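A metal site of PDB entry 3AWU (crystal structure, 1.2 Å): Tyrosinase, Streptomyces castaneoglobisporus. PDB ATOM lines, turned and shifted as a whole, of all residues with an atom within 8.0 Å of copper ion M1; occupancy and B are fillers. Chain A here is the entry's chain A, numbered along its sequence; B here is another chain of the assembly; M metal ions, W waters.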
ATOM      1  N   HIS A  38      25.340  21.403 -32.324  1.00  0.00           N
ATOM      2  CA  HIS A  38      24.427  21.960 -31.344  1.00  0.00           C
ATOM      3  C   HIS A  38      24.045  23.403 -31.663  1.00  0.00           C
ATOM      4  O   HIS A  38      22.874  23.774 -31.569  1.00  0.00           O
ATOM      5  CB  HIS A  38      25.149  21.908 -29.955  1.00  0.00           C
ATOM      6  CG  HIS A  38      24.168  22.250 -28.868  1.00  0.00           C
ATOM      7  ND1 HIS A  38      24.075  23.482 -28.296  1.00  0.00           N
ATOM      8  CD2 HIS A  38      23.262  21.487 -28.235  1.00  0.00           C
ATOM      9  CE1 HIS A  38      23.140  23.503 -27.349  1.00  0.00           C
ATOM     10  NE2 HIS A  38      22.647  22.288 -27.307  1.00  0.00           N
ATOM     11  N   ILE A  42      20.282  25.013 -32.047  1.00  0.00           N
ATOM     12  CA  ILE A  42      19.732  26.018 -31.122  1.00  0.00           C
ATOM     13  C   ILE A  42      19.447  27.303 -31.844  1.00  0.00           C
ATOM     14  O   ILE A  42      18.528  28.058 -31.459  1.00  0.00           O
ATOM     15  CB  ILE A  42      20.764  26.160 -29.968  1.00  0.00           C
ATOM     16  CG1 ILE A  42      20.061  26.597 -28.679  1.00  0.00           C
ATOM     17  CG2 ILE A  42      21.850  27.065 -30.415  1.00  0.00           C
ATOM     18  CD1 ILE A  42      21.026  26.413 -27.524  1.00  0.00           C
ATOM     19  N   GLY A  53      15.689  20.228 -31.465  1.00  0.00           N
ATOM     20  CA  GLY A  53      16.657  19.999 -30.401  1.00  0.00           C
ATOM     21  C   GLY A  53      16.249  20.617 -29.076  1.00  0.00           C
ATOM     22  O   GLY A  53      16.677  20.154 -28.013  1.00  0.00           O
ATOM     23  N   HIS A  54      15.483  21.686 -29.123  1.00  0.00           N
ATOM     24  CA  HIS A  54      15.140  22.582 -28.022  1.00  0.00           C
ATOM     25  C   HIS A  54      13.669  22.965 -28.121  1.00  0.00           C
ATOM     26  O   HIS A  54      13.037  22.805 -29.167  1.00  0.00           O
ATOM     27  CB  HIS A  54      16.001  23.877 -28.069  1.00  0.00           C
ATOM     28  CG  HIS A  54      17.460  23.510 -28.046  1.00  0.00           C
ATOM     29  ND1 HIS A  54      18.202  23.214 -29.158  1.00  0.00           N
ATOM     30  CD2 HIS A  54      18.286  23.323 -26.969  1.00  0.00           C
ATOM     31  CE1 HIS A  54      19.432  22.906 -28.749  1.00  0.00           C
ATOM     32  NE2 HIS A  54      19.536  22.957 -27.437  1.00  0.00           N
ATOM     33  N   PHE A  59      13.291  17.836 -27.165  1.00  0.00           N
ATOM     34  CA  PHE A  59      14.426  18.325 -26.381  1.00  0.00           C
ATOM     35  C   PHE A  59      15.100  17.166 -25.646  1.00  0.00           C
ATOM     36  O   PHE A  59      16.348  17.025 -25.698  1.00  0.00           O
ATOM     37  CB  PHE A  59      13.952  19.366 -25.392  1.00  0.00           C
ATOM     38  CG  PHE A  59      14.951  19.759 -24.291  1.00  0.00           C
ATOM     39  CD1 PHE A  59      16.124  20.426 -24.608  1.00  0.00           C
ATOM     40  CD2 PHE A  59      14.672  19.488 -22.956  1.00  0.00           C
ATOM     41  CE1 PHE A  59      16.995  20.827 -23.609  1.00  0.00           C
ATOM     42  CE2 PHE A  59      15.550  19.844 -21.950  1.00  0.00           C
ATOM     43  CZ  PHE A  59      16.708  20.514 -22.290  1.00  0.00           C
ATOM     44  N   HIS A  63      18.605  15.388 -27.020  1.00  0.00           N
ATOM     45  CA  HIS A  63      19.853  15.466 -26.234  1.00  0.00           C
ATOM     46  C   HIS A  63      20.296  14.102 -25.760  1.00  0.00           C
ATOM     47  O   HIS A  63      21.498  13.866 -25.614  1.00  0.00           O
ATOM     48  CB  HIS A  63      19.670  16.413 -25.039  1.00  0.00           C
ATOM     49  CG  HIS A  63      19.804  17.861 -25.483  1.00  0.00           C
ATOM     50  ND1 HIS A  63      18.759  18.613 -26.026  1.00  0.00           N
ATOM     51  CD2 HIS A  63      20.889  18.688 -25.564  1.00  0.00           C
ATOM     52  CE1 HIS A  63      19.200  19.839 -26.364  1.00  0.00           C
ATOM     53  NE2 HIS A  63      20.503  19.932 -26.080  1.00  0.00           N
ATOM     54  N   GLU A 182      13.141  21.905 -18.990  1.00  0.00           N
ATOM     55  CA  GLU A 182      13.970  22.728 -19.863  1.00  0.00           C
ATOM     56  C   GLU A 182      14.199  24.115 -19.281  1.00  0.00           C
ATOM     57  O   GLU A 182      15.291  24.655 -19.227  1.00  0.00           O
ATOM     58  CB  GLU A 182      13.313  22.768 -21.261  1.00  0.00           C
ATOM     59  CG  GLU A 182      14.256  23.421 -22.294  1.00  0.00           C
ATOM     60  CD  GLU A 182      13.730  23.385 -23.711  1.00  0.00           C
ATOM     61  OE1 GLU A 182      12.684  22.744 -24.009  1.00  0.00           O
ATOM     62  OE2 GLU A 182      14.416  23.990 -24.564  1.00  0.00           O
ATOM     63  N   HIS A 190      16.948  23.541 -16.297  1.00  0.00           N
ATOM     64  CA  HIS A 190      18.085  23.432 -17.207  1.00  0.00           C
ATOM     65  C   HIS A 190      18.606  24.739 -17.725  1.00  0.00           C
ATOM     66  O   HIS A 190      19.814  24.929 -17.844  1.00  0.00           O
ATOM     67  CB  HIS A 190      17.655  22.481 -18.384  1.00  0.00           C
ATOM     68  CG  HIS A 190      18.313  22.737 -19.697  1.00  0.00           C
ATOM     69  ND1 HIS A 190      17.843  23.702 -20.577  1.00  0.00           N
ATOM     70  CD2 HIS A 190      19.384  22.179 -20.297  1.00  0.00           C
ATOM     71  CE1 HIS A 190      18.617  23.703 -21.679  1.00  0.00           C
ATOM     72  NE2 HIS A 190      19.557  22.819 -21.522  1.00  0.00           N
ATOM     73  N   ASN A 191      17.709  25.682 -18.107  1.00  0.00           N
ATOM     74  CA  ASN A 191      18.209  26.964 -18.665  1.00  0.00           C
ATOM     75  C   ASN A 191      18.992  27.722 -17.597  1.00  0.00           C
ATOM     76  O   ASN A 191      20.055  28.295 -17.903  1.00  0.00           O
ATOM     77  CB  ASN A 191      17.061  27.816 -19.173  1.00  0.00           C
ATOM     78  CG  ASN A 191      16.463  27.377 -20.482  1.00  0.00           C
ATOM     79  OD1 ASN A 191      16.905  26.435 -21.151  1.00  0.00           O
ATOM     80  ND2 ASN A 191      15.351  28.031 -20.839  1.00  0.00           N
ATOM     81  N   VAL A 193      20.787  26.577 -15.176  1.00  0.00           N
ATOM     82  CA  VAL A 193      22.143  26.089 -14.980  1.00  0.00           C
ATOM     83  C   VAL A 193      23.098  26.646 -16.056  1.00  0.00           C
ATOM     84  O   VAL A 193      24.234  27.024 -15.743  1.00  0.00           O
ATOM     85  CB  VAL A 193      22.149  24.560 -14.992  1.00  0.00           C
ATOM     86  CG1 VAL A 193      23.593  23.996 -14.895  1.00  0.00           C
ATOM     87  CG2 VAL A 193      21.335  23.964 -13.841  1.00  0.00           C
ATOM     88  N   HIS A 194      22.651  26.698 -17.328  1.00  0.00           N
ATOM     89  CA  HIS A 194      23.454  27.320 -18.359  1.00  0.00           C
ATOM     90  C   HIS A 194      23.835  28.775 -17.988  1.00  0.00           C
ATOM     91  O   HIS A 194      24.968  29.202 -18.092  1.00  0.00           O
ATOM     92  CB  HIS A 194      22.769  27.352 -19.723  1.00  0.00           C
ATOM     93  CG  HIS A 194      22.768  26.075 -20.510  1.00  0.00           C
ATOM     94  ND1 HIS A 194      23.858  25.775 -21.324  1.00  0.00           N
ATOM     95  CD2 HIS A 194      21.856  25.109 -20.692  1.00  0.00           C
ATOM     96  CE1 HIS A 194      23.555  24.625 -21.943  1.00  0.00           C
ATOM     97  NE2 HIS A 194      22.352  24.173 -21.592  1.00  0.00           N
ATOM     98  N   MET A 201      29.044  28.480 -21.894  1.00  0.00           N
ATOM     99  CA  MET A 201      27.869  27.685 -21.487  1.00  0.00           C
ATOM    100  C   MET A 201      26.597  28.484 -21.546  1.00  0.00           C
ATOM    101  O   MET A 201      25.511  27.863 -21.620  1.00  0.00           O
ATOM    102  CB  MET A 201      28.125  27.183 -20.087  1.00  0.00           C
ATOM    103  CG  MET A 201      28.160  25.814 -19.762  1.00  0.00           C
ATOM    104  SD  MET A 201      27.261  24.537 -20.571  1.00  0.00           S
ATOM    105  CE  MET A 201      26.066  23.979 -19.362  1.00  0.00           C
ATOM    106  N   THR A 203      25.773  30.478 -24.004  1.00  0.00           N
ATOM    107  CA  THR A 203      25.656  30.882 -25.387  1.00  0.00           C
ATOM    108  C   THR A 203      25.202  29.726 -26.281  1.00  0.00           C
ATOM    109  O   THR A 203      25.095  28.589 -25.821  1.00  0.00           O
ATOM    110  CB  THR A 203      26.956  31.432 -25.969  1.00  0.00           C
ATOM    111  OG1 THR A 203      27.851  30.311 -26.241  1.00  0.00           O
ATOM    112  CG2 THR A 203      27.622  32.404 -25.030  1.00  0.00           C
ATOM    113  N   SER A 206      27.431  26.369 -26.398  1.00  0.00           N
ATOM    114  CA  SER A 206      27.650  25.909 -25.028  1.00  0.00           C
ATOM    115  C   SER A 206      28.405  24.591 -24.941  1.00  0.00           C
ATOM    116  O   SER A 206      29.104  24.449 -23.920  1.00  0.00           O
ATOM    117  CB  SER A 206      26.290  25.827 -24.298  1.00  0.00           C
ATOM    118  OG  SER A 206      25.361  25.019 -24.987  1.00  0.00           O
ATOM    119  N   PRO A 207      28.421  23.661 -25.881  1.00  0.00           N
ATOM    120  CA  PRO A 207      29.287  22.474 -25.742  1.00  0.00           C
ATOM    121  C   PRO A 207      30.763  22.815 -25.783  1.00  0.00           C
ATOM    122  O   PRO A 207      31.589  21.912 -25.554  1.00  0.00           O
ATOM    123  CB  PRO A 207      28.877  21.528 -26.889  1.00  0.00           C
ATOM    124  CG  PRO A 207      27.467  21.959 -27.183  1.00  0.00           C
ATOM    125  CD  PRO A 207      27.477  23.458 -27.032  1.00  0.00           C
ATOM    126  N   PHE A 212      29.056  21.028 -20.250  1.00  0.00           N
ATOM    127  CA  PHE A 212      27.826  20.811 -20.986  1.00  0.00           C
ATOM    128  C   PHE A 212      27.332  19.381 -20.880  1.00  0.00           C
ATOM    129  O   PHE A 212      26.159  19.128 -20.707  1.00  0.00           O
ATOM    130  CB  PHE A 212      28.090  21.197 -22.468  1.00  0.00           C
ATOM    131  CG  PHE A 212      26.923  20.912 -23.380  1.00  0.00           C
ATOM    132  CD1 PHE A 212      26.779  19.674 -24.010  1.00  0.00           C
ATOM    133  CD2 PHE A 212      25.982  21.911 -23.591  1.00  0.00           C
ATOM    134  CE1 PHE A 212      25.676  19.394 -24.810  1.00  0.00           C
ATOM    135  CE2 PHE A 212      24.898  21.663 -24.409  1.00  0.00           C
ATOM    136  CZ  PHE A 212      24.719  20.395 -25.028  1.00  0.00           C
ATOM    137  N   HIS A 215      26.102  18.448 -17.328  1.00  0.00           N
ATOM    138  CA  HIS A 215      24.786  19.037 -17.099  1.00  0.00           C
ATOM    139  C   HIS A 215      23.725  18.247 -17.844  1.00  0.00           C
ATOM    140  O   HIS A 215      22.697  17.816 -17.258  1.00  0.00           O
ATOM    141  CB  HIS A 215      24.847  20.484 -17.632  1.00  0.00           C
ATOM    142  CG  HIS A 215      23.516  21.173 -17.637  1.00  0.00           C
ATOM    143  ND1 HIS A 215      22.595  20.996 -16.644  1.00  0.00           N
ATOM    144  CD2 HIS A 215      23.010  22.109 -18.488  1.00  0.00           C
ATOM    145  CE1 HIS A 215      21.568  21.766 -16.858  1.00  0.00           C
ATOM    146  NE2 HIS A 215      21.748  22.443 -17.974  1.00  0.00           N
ATOM    147  N   HIS A 216      23.923  18.015 -19.145  1.00  0.00           N
ATOM    148  CA  HIS A 216      22.889  17.299 -19.892  1.00  0.00           C
ATOM    149  C   HIS A 216      22.771  15.868 -19.447  1.00  0.00           C
ATOM    150  O   HIS A 216      21.662  15.295 -19.570  1.00  0.00           O
ATOM    151  CB  HIS A 216      23.093  17.428 -21.438  1.00  0.00           C
ATOM    152  CG  HIS A 216      22.396  18.662 -21.904  1.00  0.00           C
ATOM    153  ND1 HIS A 216      21.020  18.626 -22.168  1.00  0.00           N
ATOM    154  CD2 HIS A 216      22.786  19.944 -22.118  1.00  0.00           C
ATOM    155  CE1 HIS A 216      20.649  19.843 -22.510  1.00  0.00           C
ATOM    156  NE2 HIS A 216      21.694  20.672 -22.505  1.00  0.00           N
ATOM    157  N   VAL A 219      20.279  16.257 -16.643  1.00  0.00           N
ATOM    158  CA  VAL A 219      18.942  16.489 -17.202  1.00  0.00           C
ATOM    159  C   VAL A 219      18.349  15.180 -17.714  1.00  0.00           C
ATOM    160  O   VAL A 219      17.176  14.885 -17.528  1.00  0.00           O
ATOM    161  CB  VAL A 219      19.061  17.559 -18.313  1.00  0.00           C
ATOM    162  CG1 VAL A 219      17.746  17.738 -19.078  1.00  0.00           C
ATOM    163  CG2 VAL A 219      19.506  18.904 -17.742  1.00  0.00           C
ATOM    164  N   HIS B  97      21.596  32.764 -24.826  1.00  0.00           N
ATOM    165  CA  HIS B  97      20.499  32.026 -25.424  1.00  0.00           C
ATOM    166  C   HIS B  97      19.535  31.478 -24.400  1.00  0.00           C
ATOM    167  O   HIS B  97      18.430  31.056 -24.780  1.00  0.00           O
ATOM    168  CB  HIS B  97      21.147  30.841 -26.186  1.00  0.00           C
ATOM    169  CG  HIS B  97      20.031  30.141 -26.877  1.00  0.00           C
ATOM    170  ND1 HIS B  97      19.512  30.547 -28.074  1.00  0.00           N
ATOM    171  CD2 HIS B  97      19.315  29.040 -26.566  1.00  0.00           C
ATOM    172  CE1 HIS B  97      18.538  29.747 -28.453  1.00  0.00           C
ATOM    173  NE2 HIS B  97      18.385  28.809 -27.560  1.00  0.00           N
ATOM    174  N   TYR B  98      19.905  31.412 -23.129  1.00  0.00           N
ATOM    175  CA  TYR B  98      19.081  30.698 -22.155  1.00  0.00           C
ATOM    176  C   TYR B  98      18.465  31.673 -21.173  1.00  0.00           C
ATOM    177  O   TYR B  98      17.958  31.253 -20.129  1.00  0.00           O
ATOM    178  CB  TYR B  98      19.989  29.688 -21.447  1.00  0.00           C
ATOM    179  CG  TYR B  98      20.565  28.628 -22.370  1.00  0.00           C
ATOM    180  CD1 TYR B  98      21.865  28.807 -22.822  1.00  0.00           C
ATOM    181  CD2 TYR B  98      19.886  27.476 -22.767  1.00  0.00           C
ATOM    182  CE1 TYR B  98      22.470  27.880 -23.672  1.00  0.00           C
ATOM    183  CE2 TYR B  98      20.500  26.540 -23.600  1.00  0.00           C
ATOM    184  CZ  TYR B  98      21.803  26.733 -24.052  1.00  0.00           C
ATOM    185  OH  TYR B  98      22.391  25.810 -24.892  1.00  0.00           O
HETATM  186 CU    CU M   1      21.255  22.763 -22.634  1.00  0.00          CU
HETATM  187 CU    CU M   2      20.918  22.641 -26.025  1.00  0.00          CU
HETATM  188  O   HOH W   1      19.498  23.165 -24.427  1.00  0.00           O
HETATM  189  O   HOH W   2      21.771  23.065 -24.426  1.00  0.00           O
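Copper ion M1 is bound by water W2 (1.9 Å), NE2 of His 190 (2.0 Å), NE2 of His 194 (2.1 Å), NE2 of His 216 (2.1 Å) and water W1 (2.5 Å).
The backbone carbonyl oxygen of His 190 sits at hydrogen-bond distance from a ring nitrogen (NE2) of His 215 (3.2 Å). ND1 of His 190 is in hydrogen-bond range of OD1 of Asn 191 (2.9 Å). The backbone carbonyl oxygen (O) of Glu 182 sits at hydrogen-bond distance from a ring nitrogen (ND1) of His 190. A ring nitrogen (ND1) of His 194 lies within hydrogen-bond range of the backbone carbonyl oxygen (O) of Met 201, 2.7 Å away. The side-chain hydroxyl (OH) of Tyr 98 of chain B sits at hydrogen-bond distance from the side-chain hydroxyl (OG) of Ser 206 (3.1 Å).
Merely in contact with copper ion M1: Tyr 98 of chain B (3.96 Å). Of the 21 residues printed, 4 come within 4 Å of copper ion M1. The nearest printed residue that does not touch copper ion M1 is Phe 212 (4.2 Å).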
